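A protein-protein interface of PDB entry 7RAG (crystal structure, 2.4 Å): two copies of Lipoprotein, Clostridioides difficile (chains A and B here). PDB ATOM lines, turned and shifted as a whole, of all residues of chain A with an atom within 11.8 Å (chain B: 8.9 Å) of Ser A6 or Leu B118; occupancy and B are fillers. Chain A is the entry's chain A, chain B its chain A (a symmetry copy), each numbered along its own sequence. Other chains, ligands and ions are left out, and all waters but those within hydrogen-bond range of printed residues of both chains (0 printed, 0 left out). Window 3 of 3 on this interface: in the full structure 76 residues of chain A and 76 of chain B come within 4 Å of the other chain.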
ATOM      1  N   GLN A   2     -17.792  36.334 -31.103  1.00  0.00           N
ATOM      2  CA  GLN A   2     -17.062  35.176 -30.629  1.00  0.00           C
ATOM      3  C   GLN A   2     -17.709  34.681 -29.338  1.00  0.00           C
ATOM      4  O   GLN A   2     -18.478  35.397 -28.698  1.00  0.00           O
ATOM      5  CB  GLN A   2     -15.576  35.557 -30.484  1.00  0.00           C
ATOM      6  CG  GLN A   2     -14.792  34.947 -29.349  1.00  0.00           C
ATOM      7  CD  GLN A   2     -13.577  35.791 -29.002  1.00  0.00           C
ATOM      8  OE1 GLN A   2     -13.718  36.916 -28.515  1.00  0.00           O
ATOM      9  NE2 GLN A   2     -12.376  35.261 -29.266  1.00  0.00           N
ATOM     10  N   LYS A   3     -17.431  33.424 -28.986  1.00  0.00           N
ATOM     11  CA  LYS A   3     -18.005  32.830 -27.785  1.00  0.00           C
ATOM     12  C   LYS A   3     -17.477  33.517 -26.520  1.00  0.00           C
ATOM     13  O   LYS A   3     -16.492  34.267 -26.540  1.00  0.00           O
ATOM     14  CB  LYS A   3     -17.709  31.329 -27.730  1.00  0.00           C
ATOM     15  CG  LYS A   3     -18.592  30.522 -28.651  1.00  0.00           C
ATOM     16  CD  LYS A   3     -18.351  29.019 -28.595  1.00  0.00           C
ATOM     17  CE  LYS A   3     -19.375  28.348 -29.527  1.00  0.00           C
ATOM     18  NZ  LYS A   3     -19.207  26.875 -29.674  1.00  0.00           N
ATOM     19  N   ARG A   4     -18.155  33.247 -25.404  1.00  0.00           N
ATOM     20  CA  ARG A   4     -17.756  33.781 -24.111  1.00  0.00           C
ATOM     21  C   ARG A   4     -16.508  33.068 -23.613  1.00  0.00           C
ATOM     22  O   ARG A   4     -16.219  31.932 -23.999  1.00  0.00           O
ATOM     23  CB  ARG A   4     -18.876  33.627 -23.078  1.00  0.00           C
ATOM     24  CG  ARG A   4     -19.067  32.192 -22.623  1.00  0.00           C
ATOM     25  CD  ARG A   4     -20.041  32.058 -21.446  1.00  0.00           C
ATOM     26  NE  ARG A   4     -20.362  30.655 -21.179  1.00  0.00           N
ATOM     27  CZ  ARG A   4     -19.563  29.809 -20.533  1.00  0.00           C
ATOM     28  NH1 ARG A   4     -18.382  30.213 -20.076  1.00  0.00           N
ATOM     29  NH2 ARG A   4     -19.947  28.552 -20.353  1.00  0.00           N
ATOM     30  N   GLN A   5     -15.766  33.753 -22.740  1.00  0.00           N
ATOM     31  CA  GLN A   5     -14.565  33.170 -22.156  1.00  0.00           C
ATOM     32  C   GLN A   5     -14.896  31.895 -21.393  1.00  0.00           C
ATOM     33  O   GLN A   5     -15.881  31.828 -20.650  1.00  0.00           O
ATOM     34  CB  GLN A   5     -13.888  34.171 -21.221  1.00  0.00           C
ATOM     35  CG  GLN A   5     -13.620  35.510 -21.869  1.00  0.00           C
ATOM     36  CD  GLN A   5     -13.086  35.366 -23.286  1.00  0.00           C
ATOM     37  OE1 GLN A   5     -12.060  34.713 -23.512  1.00  0.00           O
ATOM     38  NE2 GLN A   5     -13.788  35.970 -24.257  1.00  0.00           N
ATOM     39  N   SER A   6     -14.080  30.872 -21.589  1.00  0.00           N
ATOM     40  CA  SER A   6     -14.241  29.667 -20.804  1.00  0.00           C
ATOM     41  C   SER A   6     -13.891  29.953 -19.353  1.00  0.00           C
ATOM     42  O   SER A   6     -12.991  30.747 -19.058  1.00  0.00           O
ATOM     43  CB  SER A   6     -13.368  28.556 -21.358  1.00  0.00           C
ATOM     44  OG  SER A   6     -13.817  28.202 -22.645  1.00  0.00           O
ATOM     45  N   THR A   7     -14.637  29.325 -18.448  1.00  0.00           N
ATOM     46  CA  THR A   7     -14.343  29.356 -17.023  1.00  0.00           C
ATOM     47  C   THR A   7     -13.166  28.438 -16.711  1.00  0.00           C
ATOM     48  O   THR A   7     -12.659  27.710 -17.570  1.00  0.00           O
ATOM     49  CB  THR A   7     -15.558  28.920 -16.208  1.00  0.00           C
ATOM     50  OG1 THR A   7     -15.739  27.509 -16.366  1.00  0.00           O
ATOM     51  CG2 THR A   7     -16.799  29.641 -16.676  1.00  0.00           C
ATOM     52  N   LYS A   8     -12.748  28.451 -15.447  1.00  0.00           N
ATOM     53  CA  LYS A   8     -11.664  27.581 -15.015  1.00  0.00           C
ATOM     54  C   LYS A   8     -11.946  26.123 -15.349  1.00  0.00           C
ATOM     55  O   LYS A   8     -11.108  25.423 -15.936  1.00  0.00           O
ATOM     56  CB  LYS A   8     -11.434  27.742 -13.511  1.00  0.00           C
ATOM     57  CG  LYS A   8     -10.357  28.719 -13.165  1.00  0.00           C
ATOM     58  CD  LYS A   8      -8.981  28.068 -13.250  1.00  0.00           C
ATOM     59  CE  LYS A   8      -8.514  27.747 -14.689  1.00  0.00           C
ATOM     60  NZ  LYS A   8      -7.052  27.841 -14.996  1.00  0.00           N
ATOM     61  N   GLU A   9     -13.136  25.654 -14.987  1.00  0.00           N
ATOM     62  CA  GLU A   9     -13.421  24.234 -15.094  1.00  0.00           C
ATOM     63  C   GLU A   9     -13.568  23.812 -16.545  1.00  0.00           C
ATOM     64  O   GLU A   9     -13.184  22.694 -16.903  1.00  0.00           O
ATOM     65  CB  GLU A   9     -14.678  23.891 -14.294  1.00  0.00           C
ATOM     66  CG  GLU A   9     -14.644  24.350 -12.828  1.00  0.00           C
ATOM     67  CD  GLU A   9     -15.069  25.809 -12.631  1.00  0.00           C
ATOM     68  OE1 GLU A   9     -14.370  26.710 -13.142  1.00  0.00           O
ATOM     69  OE2 GLU A   9     -16.107  26.051 -11.966  1.00  0.00           O
ATOM     70  N   GLU A  10     -14.100  24.695 -17.391  1.00  0.00           N
ATOM     71  CA  GLU A  10     -14.258  24.354 -18.801  1.00  0.00           C
ATOM     72  C   GLU A  10     -12.902  24.183 -19.478  1.00  0.00           C
ATOM     73  O   GLU A  10     -12.673  23.192 -20.186  1.00  0.00           O
ATOM     74  CB  GLU A  10     -15.100  25.420 -19.508  1.00  0.00           C
ATOM     75  CG  GLU A  10     -16.422  25.731 -18.811  1.00  0.00           C
ATOM     76  CD  GLU A  10     -17.339  26.630 -19.625  1.00  0.00           C
ATOM     77  OE1 GLU A  10     -18.492  26.205 -19.888  1.00  0.00           O
ATOM     78  OE2 GLU A  10     -16.910  27.751 -20.007  1.00  0.00           O
ATOM     79  N   VAL A  11     -11.978  25.125 -19.244  1.00  0.00           N
ATOM     80  CA  VAL A  11     -10.628  24.998 -19.790  1.00  0.00           C
ATOM     81  C   VAL A  11      -9.947  23.757 -19.236  1.00  0.00           C
ATOM     82  O   VAL A  11      -9.306  22.996 -19.976  1.00  0.00           O
ATOM     83  CB  VAL A  11      -9.799  26.265 -19.501  1.00  0.00           C
ATOM     84  CG1 VAL A  11      -8.332  26.003 -19.783  1.00  0.00           C
ATOM     85  CG2 VAL A  11     -10.266  27.430 -20.354  1.00  0.00           C
ATOM     86  N   TYR A  12     -10.080  23.526 -17.928  1.00  0.00           N
ATOM     87  CA  TYR A  12      -9.422  22.377 -17.319  1.00  0.00           C
ATOM     88  C   TYR A  12      -9.936  21.064 -17.895  1.00  0.00           C
ATOM     89  O   TYR A  12      -9.149  20.147 -18.170  1.00  0.00           O
ATOM     90  CB  TYR A  12      -9.610  22.406 -15.805  1.00  0.00           C
ATOM     91  CG  TYR A  12      -8.990  21.212 -15.128  1.00  0.00           C
ATOM     92  CD1 TYR A  12      -9.767  20.303 -14.425  1.00  0.00           C
ATOM     93  CD2 TYR A  12      -7.623  20.976 -15.222  1.00  0.00           C
ATOM     94  CE1 TYR A  12      -9.196  19.201 -13.814  1.00  0.00           C
ATOM     95  CE2 TYR A  12      -7.042  19.888 -14.614  1.00  0.00           C
ATOM     96  CZ  TYR A  12      -7.831  18.997 -13.910  1.00  0.00           C
ATOM     97  OH  TYR A  12      -7.250  17.900 -13.303  1.00  0.00           O
ATOM     98  N   LYS A  13     -11.253  20.951 -18.087  1.00  0.00           N
ATOM     99  CA  LYS A  13     -11.809  19.712 -18.624  1.00  0.00           C
ATOM    100  C   LYS A  13     -11.435  19.537 -20.087  1.00  0.00           C
ATOM    101  O   LYS A  13     -11.165  18.414 -20.535  1.00  0.00           O
ATOM    102  CB  LYS A  13     -13.324  19.678 -18.439  1.00  0.00           C
ATOM    103  CG  LYS A  13     -13.923  18.282 -18.577  1.00  0.00           C
ATOM    104  CD  LYS A  13     -15.437  18.324 -18.454  1.00  0.00           C
ATOM    105  N   ASP A  14     -11.382  20.637 -20.842  1.00  0.00           N
ATOM    106  CA  ASP A  14     -10.878  20.545 -22.210  1.00  0.00           C
ATOM    107  C   ASP A  14      -9.454  20.002 -22.221  1.00  0.00           C
ATOM    108  O   ASP A  14      -9.126  19.114 -23.017  1.00  0.00           O
ATOM    109  CB  ASP A  14     -10.952  21.914 -22.900  1.00  0.00           C
ATOM    110  CG  ASP A  14     -12.383  22.360 -23.186  1.00  0.00           C
ATOM    111  OD1 ASP A  14     -13.308  21.541 -23.013  1.00  0.00           O
ATOM    112  OD2 ASP A  14     -12.591  23.529 -23.580  1.00  0.00           O
ATOM    113  N   PHE A  15      -8.607  20.505 -21.320  1.00  0.00           N
ATOM    114  CA  PHE A  15      -7.233  20.018 -21.227  1.00  0.00           C
ATOM    115  C   PHE A  15      -7.190  18.525 -20.895  1.00  0.00           C
ATOM    116  O   PHE A  15      -6.395  17.773 -21.478  1.00  0.00           O
ATOM    117  CB  PHE A  15      -6.474  20.836 -20.178  1.00  0.00           C
ATOM    118  CG  PHE A  15      -5.126  20.270 -19.806  1.00  0.00           C
ATOM    119  CD1 PHE A  15      -4.020  20.471 -20.621  1.00  0.00           C
ATOM    120  CD2 PHE A  15      -4.955  19.556 -18.621  1.00  0.00           C
ATOM    121  CE1 PHE A  15      -2.765  19.953 -20.273  1.00  0.00           C
ATOM    122  CE2 PHE A  15      -3.707  19.035 -18.268  1.00  0.00           C
ATOM    123  CZ  PHE A  15      -2.610  19.232 -19.099  1.00  0.00           C
ATOM    124  N   GLN A  18      -8.046  16.586 -23.950  1.00  0.00           N
ATOM    125  CA  GLN A  18      -6.986  16.645 -24.949  1.00  0.00           C
ATOM    126  C   GLN A  18      -5.835  15.718 -24.587  1.00  0.00           C
ATOM    127  O   GLN A  18      -5.340  14.973 -25.435  1.00  0.00           O
ATOM    128  CB  GLN A  18      -6.491  18.089 -25.116  1.00  0.00           C
ATOM    129  CG  GLN A  18      -5.449  18.243 -26.225  1.00  0.00           C
ATOM    130  CD  GLN A  18      -5.285  19.673 -26.725  1.00  0.00           C
ATOM    131  OE1 GLN A  18      -6.267  20.365 -27.020  1.00  0.00           O
ATOM    132  NE2 GLN A  18      -4.033  20.122 -26.824  1.00  0.00           N
ATOM    133  N   LYS B 115      -4.916  22.670  -6.999  1.00  0.00           N
ATOM    134  CA  LYS B 115      -5.254  24.086  -7.172  1.00  0.00           C
ATOM    135  C   LYS B 115      -5.298  24.422  -8.659  1.00  0.00           C
ATOM    136  O   LYS B 115      -4.303  24.239  -9.370  1.00  0.00           O
ATOM    137  CB  LYS B 115      -4.235  24.990  -6.468  1.00  0.00           C
ATOM    138  CG  LYS B 115      -4.484  25.257  -4.983  1.00  0.00           C
ATOM    139  N   VAL B 116      -6.438  24.936  -9.124  1.00  0.00           N
ATOM    140  CA  VAL B 116      -6.621  25.345 -10.516  1.00  0.00           C
ATOM    141  C   VAL B 116      -6.909  26.842 -10.547  1.00  0.00           C
ATOM    142  O   VAL B 116      -7.779  27.324  -9.815  1.00  0.00           O
ATOM    143  CB  VAL B 116      -7.748  24.551 -11.205  1.00  0.00           C
ATOM    144  CG1 VAL B 116      -7.756  24.831 -12.671  1.00  0.00           C
ATOM    145  CG2 VAL B 116      -7.557  23.068 -10.986  1.00  0.00           C
ATOM    146  N   LYS B 117      -6.172  27.572 -11.391  1.00  0.00           N
ATOM    147  CA  LYS B 117      -6.225  29.032 -11.454  1.00  0.00           C
ATOM    148  C   LYS B 117      -6.116  29.481 -12.910  1.00  0.00           C
ATOM    149  O   LYS B 117      -5.412  28.854 -13.700  1.00  0.00           O
ATOM    150  CB  LYS B 117      -5.099  29.644 -10.606  1.00  0.00           C
ATOM    151  CG  LYS B 117      -4.792  31.100 -10.880  1.00  0.00           C
ATOM    152  CD  LYS B 117      -3.362  31.426 -10.474  1.00  0.00           C
ATOM    153  CE  LYS B 117      -3.000  30.785  -9.141  1.00  0.00           C
ATOM    154  NZ  LYS B 117      -1.650  31.191  -8.665  1.00  0.00           N
ATOM    155  N   LEU B 118      -6.860  30.522 -13.292  1.00  0.00           N
ATOM    156  CA  LEU B 118      -6.884  31.014 -14.675  1.00  0.00           C
ATOM    157  C   LEU B 118      -6.273  32.410 -14.668  1.00  0.00           C
ATOM    158  O   LEU B 118      -6.930  33.381 -14.284  1.00  0.00           O
ATOM    159  CB  LEU B 118      -8.308  31.017 -15.224  1.00  0.00           C
ATOM    160  CG  LEU B 118      -8.629  30.947 -16.721  1.00  0.00           C
ATOM    161  CD1 LEU B 118      -7.840  29.888 -17.455  1.00  0.00           C
ATOM    162  CD2 LEU B 118     -10.096  30.668 -16.885  1.00  0.00           C
ATOM    163  N   SER B 119      -5.014  32.512 -15.080  1.00  0.00           N
ATOM    164  CA  SER B 119      -4.242  33.729 -14.860  1.00  0.00           C
ATOM    165  C   SER B 119      -3.445  34.065 -16.112  1.00  0.00           C
ATOM    166  O   SER B 119      -2.629  33.255 -16.567  1.00  0.00           O
ATOM    167  CB  SER B 119      -3.314  33.560 -13.648  1.00  0.00           C
ATOM    168  OG  SER B 119      -2.533  34.718 -13.417  1.00  0.00           O
ATOM    169  N   LYS B 120      -3.696  35.253 -16.664  1.00  0.00           N
ATOM    170  CA  LYS B 120      -2.892  35.820 -17.746  1.00  0.00           C
ATOM    171  C   LYS B 120      -2.730  34.833 -18.904  1.00  0.00           C
ATOM    172  O   LYS B 120      -1.623  34.574 -19.385  1.00  0.00           O
ATOM    173  CB  LYS B 120      -1.533  36.281 -17.215  1.00  0.00           C
ATOM    174  N   GLY B 121      -3.853  34.266 -19.344  1.00  0.00           N
ATOM    175  CA  GLY B 121      -3.837  33.343 -20.466  1.00  0.00           C
ATOM    176  C   GLY B 121      -3.297  31.957 -20.176  1.00  0.00           C
ATOM    177  O   GLY B 121      -3.001  31.207 -21.111  1.00  0.00           O
ATOM    178  N   HIS B 122      -3.172  31.583 -18.904  1.00  0.00           N
ATOM    179  CA  HIS B 122      -2.675  30.265 -18.537  1.00  0.00           C
ATOM    180  C   HIS B 122      -3.591  29.587 -17.536  1.00  0.00           C
ATOM    181  O   HIS B 122      -4.100  30.219 -16.605  1.00  0.00           O
ATOM    182  CB  HIS B 122      -1.277  30.337 -17.946  1.00  0.00           C
ATOM    183  CG  HIS B 122      -0.231  30.712 -18.939  1.00  0.00           C
ATOM    184  ND1 HIS B 122       0.145  32.019 -19.161  1.00  0.00           N
ATOM    185  CD2 HIS B 122       0.505  29.954 -19.783  1.00  0.00           C
ATOM    186  CE1 HIS B 122       1.081  32.049 -20.093  1.00  0.00           C
ATOM    187  NE2 HIS B 122       1.316  30.811 -20.489  1.00  0.00           N
ATOM    188  N   LEU B 123      -3.786  28.292 -17.747  1.00  0.00           N
ATOM    189  CA  LEU B 123      -4.354  27.395 -16.753  1.00  0.00           C
ATOM    190  C   LEU B 123      -3.200  26.952 -15.857  1.00  0.00           C
ATOM    191  O   LEU B 123      -2.256  26.325 -16.332  1.00  0.00           O
ATOM    192  CB  LEU B 123      -5.034  26.223 -17.463  1.00  0.00           C
ATOM    193  CG  LEU B 123      -5.634  24.963 -16.815  1.00  0.00           C
ATOM    194  CD1 LEU B 123      -7.065  25.139 -16.425  1.00  0.00           C
ATOM    195  CD2 LEU B 123      -5.516  23.758 -17.760  1.00  0.00           C
ATOM    196  N   VAL B 124      -3.238  27.334 -14.583  1.00  0.00           N
ATOM    197  CA  VAL B 124      -2.200  26.993 -13.614  1.00  0.00           C
ATOM    198  C   VAL B 124      -2.720  25.855 -12.754  1.00  0.00           C
ATOM    199  O   VAL B 124      -3.793  25.971 -12.145  1.00  0.00           O
ATOM    200  CB  VAL B 124      -1.816  28.200 -12.744  1.00  0.00           C
ATOM    201  CG1 VAL B 124      -0.587  27.881 -11.911  1.00  0.00           C
ATOM    202  CG2 VAL B 124      -1.571  29.418 -13.602  1.00  0.00           C
ATOM    203  N   LEU B 125      -1.961  24.757 -12.705  1.00  0.00           N
ATOM    204  CA  LEU B 125      -2.335  23.552 -11.974  1.00  0.00           C
ATOM    205  C   LEU B 125      -1.252  23.251 -10.953  1.00  0.00           C
ATOM    206  O   LEU B 125      -0.087  23.085 -11.323  1.00  0.00           O
ATOM    207  CB  LEU B 125      -2.495  22.374 -12.926  1.00  0.00           C
ATOM    208  CG  LEU B 125      -3.344  22.626 -14.163  1.00  0.00           C
ATOM    209  CD1 LEU B 125      -3.471  21.337 -14.957  1.00  0.00           C
ATOM    210  CD2 LEU B 125      -4.709  23.146 -13.765  1.00  0.00           C
ATOM    211  N   GLU B 126      -1.630  23.170  -9.679  1.00  0.00           N
ATOM    212  CA  GLU B 126      -0.682  22.966  -8.589  1.00  0.00           C
ATOM    213  C   GLU B 126      -1.035  21.711  -7.809  1.00  0.00           C
ATOM    214  O   GLU B 126      -2.171  21.556  -7.363  1.00  0.00           O
ATOM    215  CB  GLU B 126      -0.676  24.143  -7.621  1.00  0.00           C
ATOM    216  CG  GLU B 126      -0.744  25.498  -8.254  1.00  0.00           C
ATOM    217  CD  GLU B 126      -0.709  26.573  -7.197  1.00  0.00           C
ATOM    218  OE1 GLU B 126      -0.642  26.198  -5.999  1.00  0.00           O
ATOM    219  OE2 GLU B 126      -0.740  27.771  -7.562  1.00  0.00           O
ATOM    220  N   VAL B 143      -0.372  25.750 -18.408  1.00  0.00           N
ATOM    221  CA  VAL B 143      -0.945  25.294 -19.667  1.00  0.00           C
ATOM    222  C   VAL B 143      -1.436  26.514 -20.437  1.00  0.00           C
ATOM    223  O   VAL B 143      -2.035  27.426 -19.859  1.00  0.00           O
ATOM    224  CB  VAL B 143      -2.095  24.293 -19.422  1.00  0.00           C
ATOM    225  CG1 VAL B 143      -2.602  23.733 -20.747  1.00  0.00           C
ATOM    226  CG2 VAL B 143      -1.639  23.178 -18.501  1.00  0.00           C
ATOM    227  N   ASN B 144      -1.170  26.538 -21.736  1.00  0.00           N
ATOM    228  CA  ASN B 144      -1.697  27.605 -22.571  1.00  0.00           C
ATOM    229  C   ASN B 144      -3.210  27.463 -22.654  1.00  0.00           C
ATOM    230  O   ASN B 144      -3.719  26.423 -23.074  1.00  0.00           O
ATOM    231  CB  ASN B 144      -1.056  27.541 -23.953  1.00  0.00           C
ATOM    232  CG  ASN B 144      -1.511  28.651 -24.852  1.00  0.00           C
ATOM    233  OD1 ASN B 144      -2.654  28.690 -25.292  1.00  0.00           O
ATOM    234  ND2 ASN B 144      -0.610  29.555 -25.149  1.00  0.00           N
ATOM    235  N   ALA B 145      -3.937  28.503 -22.261  1.00  0.00           N
ATOM    236  CA  ALA B 145      -5.380  28.366 -22.142  1.00  0.00           C
ATOM    237  C   ALA B 145      -6.065  28.223 -23.482  1.00  0.00           C
ATOM    238  O   ALA B 145      -7.228  27.814 -23.514  1.00  0.00           O
ATOM    239  CB  ALA B 145      -5.972  29.556 -21.394  1.00  0.00           C
ATOM    240  N   ASP B 146      -5.382  28.539 -24.581  1.00  0.00           N
ATOM    241  CA  ASP B 146      -5.954  28.406 -25.914  1.00  0.00           C
ATOM    242  C   ASP B 146      -5.584  27.090 -26.583  1.00  0.00           C
ATOM    243  O   ASP B 146      -6.454  26.376 -27.084  1.00  0.00           O
ATOM    244  CB  ASP B 146      -5.494  29.572 -26.786  1.00  0.00           C
ATOM    245  CG  ASP B 146      -6.059  30.891 -26.326  1.00  0.00           C
ATOM    246  OD1 ASP B 146      -7.286  30.949 -26.104  1.00  0.00           O
ATOM    247  OD2 ASP B 146      -5.269  31.854 -26.181  1.00  0.00           O
ATOM    248  N   LYS B 148      -4.274  24.544 -24.955  1.00  0.00           N
ATOM    249  CA  LYS B 148      -4.256  23.505 -23.918  1.00  0.00           C
ATOM    250  C   LYS B 148      -2.972  22.690 -23.949  1.00  0.00           C
ATOM    251  O   LYS B 148      -2.934  21.577 -23.424  1.00  0.00           O
ATOM    252  CB  LYS B 148      -5.468  22.564 -24.017  1.00  0.00           C
ATOM    253  CG  LYS B 148      -6.757  23.234 -24.506  1.00  0.00           C
ATOM    254  CD  LYS B 148      -7.565  23.808 -23.369  1.00  0.00           C
ATOM    255  CE  LYS B 148      -8.267  25.079 -23.780  1.00  0.00           C
ATOM    256  NZ  LYS B 148      -8.858  25.018 -25.135  1.00  0.00           N
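NZ of Lys A8 sits close to N of Leu B118, at 3.2 Å. O of Lys B117 sits close to NZ of Lys A8.
The side-chain amino group (NZ) of Lys B117 is in salt-bridge range of the side-chain carboxylate (OE2) of Glu B126, 3.7 Å away. The side-chain amino group (NZ) of Lys B148 sits at hydrogen-bond distance from the backbone carbonyl oxygen (O) of Asp B146 (3.4 Å). The backbone carbonyl oxygen (O) of Lys B117 is in hydrogen-bond range of the backbone NH (N) of Val B124 (2.8 Å). The backbone NH (N) of Glu A9 sits close to the side-chain hydroxyl (OG1) of Thr A7 (3.5 Å). The backbone NH (N) of Thr A7 is in hydrogen-bond range of the side-chain carboxylate (OE2) of Glu A10 (3.2 Å). The backbone carbonyl oxygen (O) of Leu B123 lies within hydrogen-bond range of the backbone NH (N) of Val B143 (2.9 Å).
Among the printed residues, pairs that only touch across the chains: Ser A6 with Leu B118 (3.6 Å), Thr A7 with Leu B118 (3.8 Å), Lys A8 with Val B116 (3.5 Å), Lys A8 with Leu B123 (3.1 Å), Lys A8 with Val B124 (3.9 Å), Val A11 with Leu B123 (3.7 Å), Val A11 with Lys B148 (3.9 Å), Tyr A12 with Leu B123 (3.7 Å), Tyr A12 with Leu B125 (3.9 Å), Asp A14 with Lys B148 (3.9 Å), Phe A15 with Leu B123 (3.9 Å), Phe A15 with Val B143 (3.6 Å), Phe A15 with Lys B148 (3.2 Å) and Gln A18 with Lys B148 (3.8 Å).
Ser A6 touches just one residue of chain B: Leu B118 (3.6 Å). Of chain B, only Leu B118 comes within 4 Å of Thr A7. Of the printed residues of chain B, Lys A8 touches Val B116, Lys B117, Leu B118, Leu B123 and Val B124. Printed residues of chain B within 4 Å of Asp A14: Lys B148. Of the printed residues of chain B, Gln A18 touches Lys B148. Of the printed residues of chain A, Val B116 touches Lys A8. Lys B117 touches one residue of chain A. Leu B118 touches just these residues of chain A: Ser A6, Thr A7 and Lys A8. No residue of chain A comes within 4 Å of Ser B119. No residue of chain A comes within 4 Å of Lys B120. Gly B121 touches none of the printed residues of chain A. Of chain A, only Lys A8 (3.1 Å), Val A11 (3.7 Å), Tyr A12 (3.7 Å) and Phe A15 (3.9 Å) come within 4 Å of Leu B123. Printed residues of chain A within 4 Å of Val B124: Lys A8. Of the printed residues of chain A, Val B143 touches Phe A15. No residue of chain A comes within 4 Å of Ala B145.
Of the 15 printed residues of chain A, 8 touch a printed residue of chain B. Hydrophobic or aromatic side chains of chain A that line the printed part of chain B: Val A11, Tyr A12 and Phe A15. Hydrophobic or aromatic side chains of chain B that line the printed part of chain A: Val B116, Leu B118, Leu B123, Leu B125 and Val B143. Among the printed residues, 16 pairs touch across the chains.
No position is printed for both chains. Of the 16 pairs that touch across the chains among the printed residues, none has its exchanged pair printed and touching as well.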
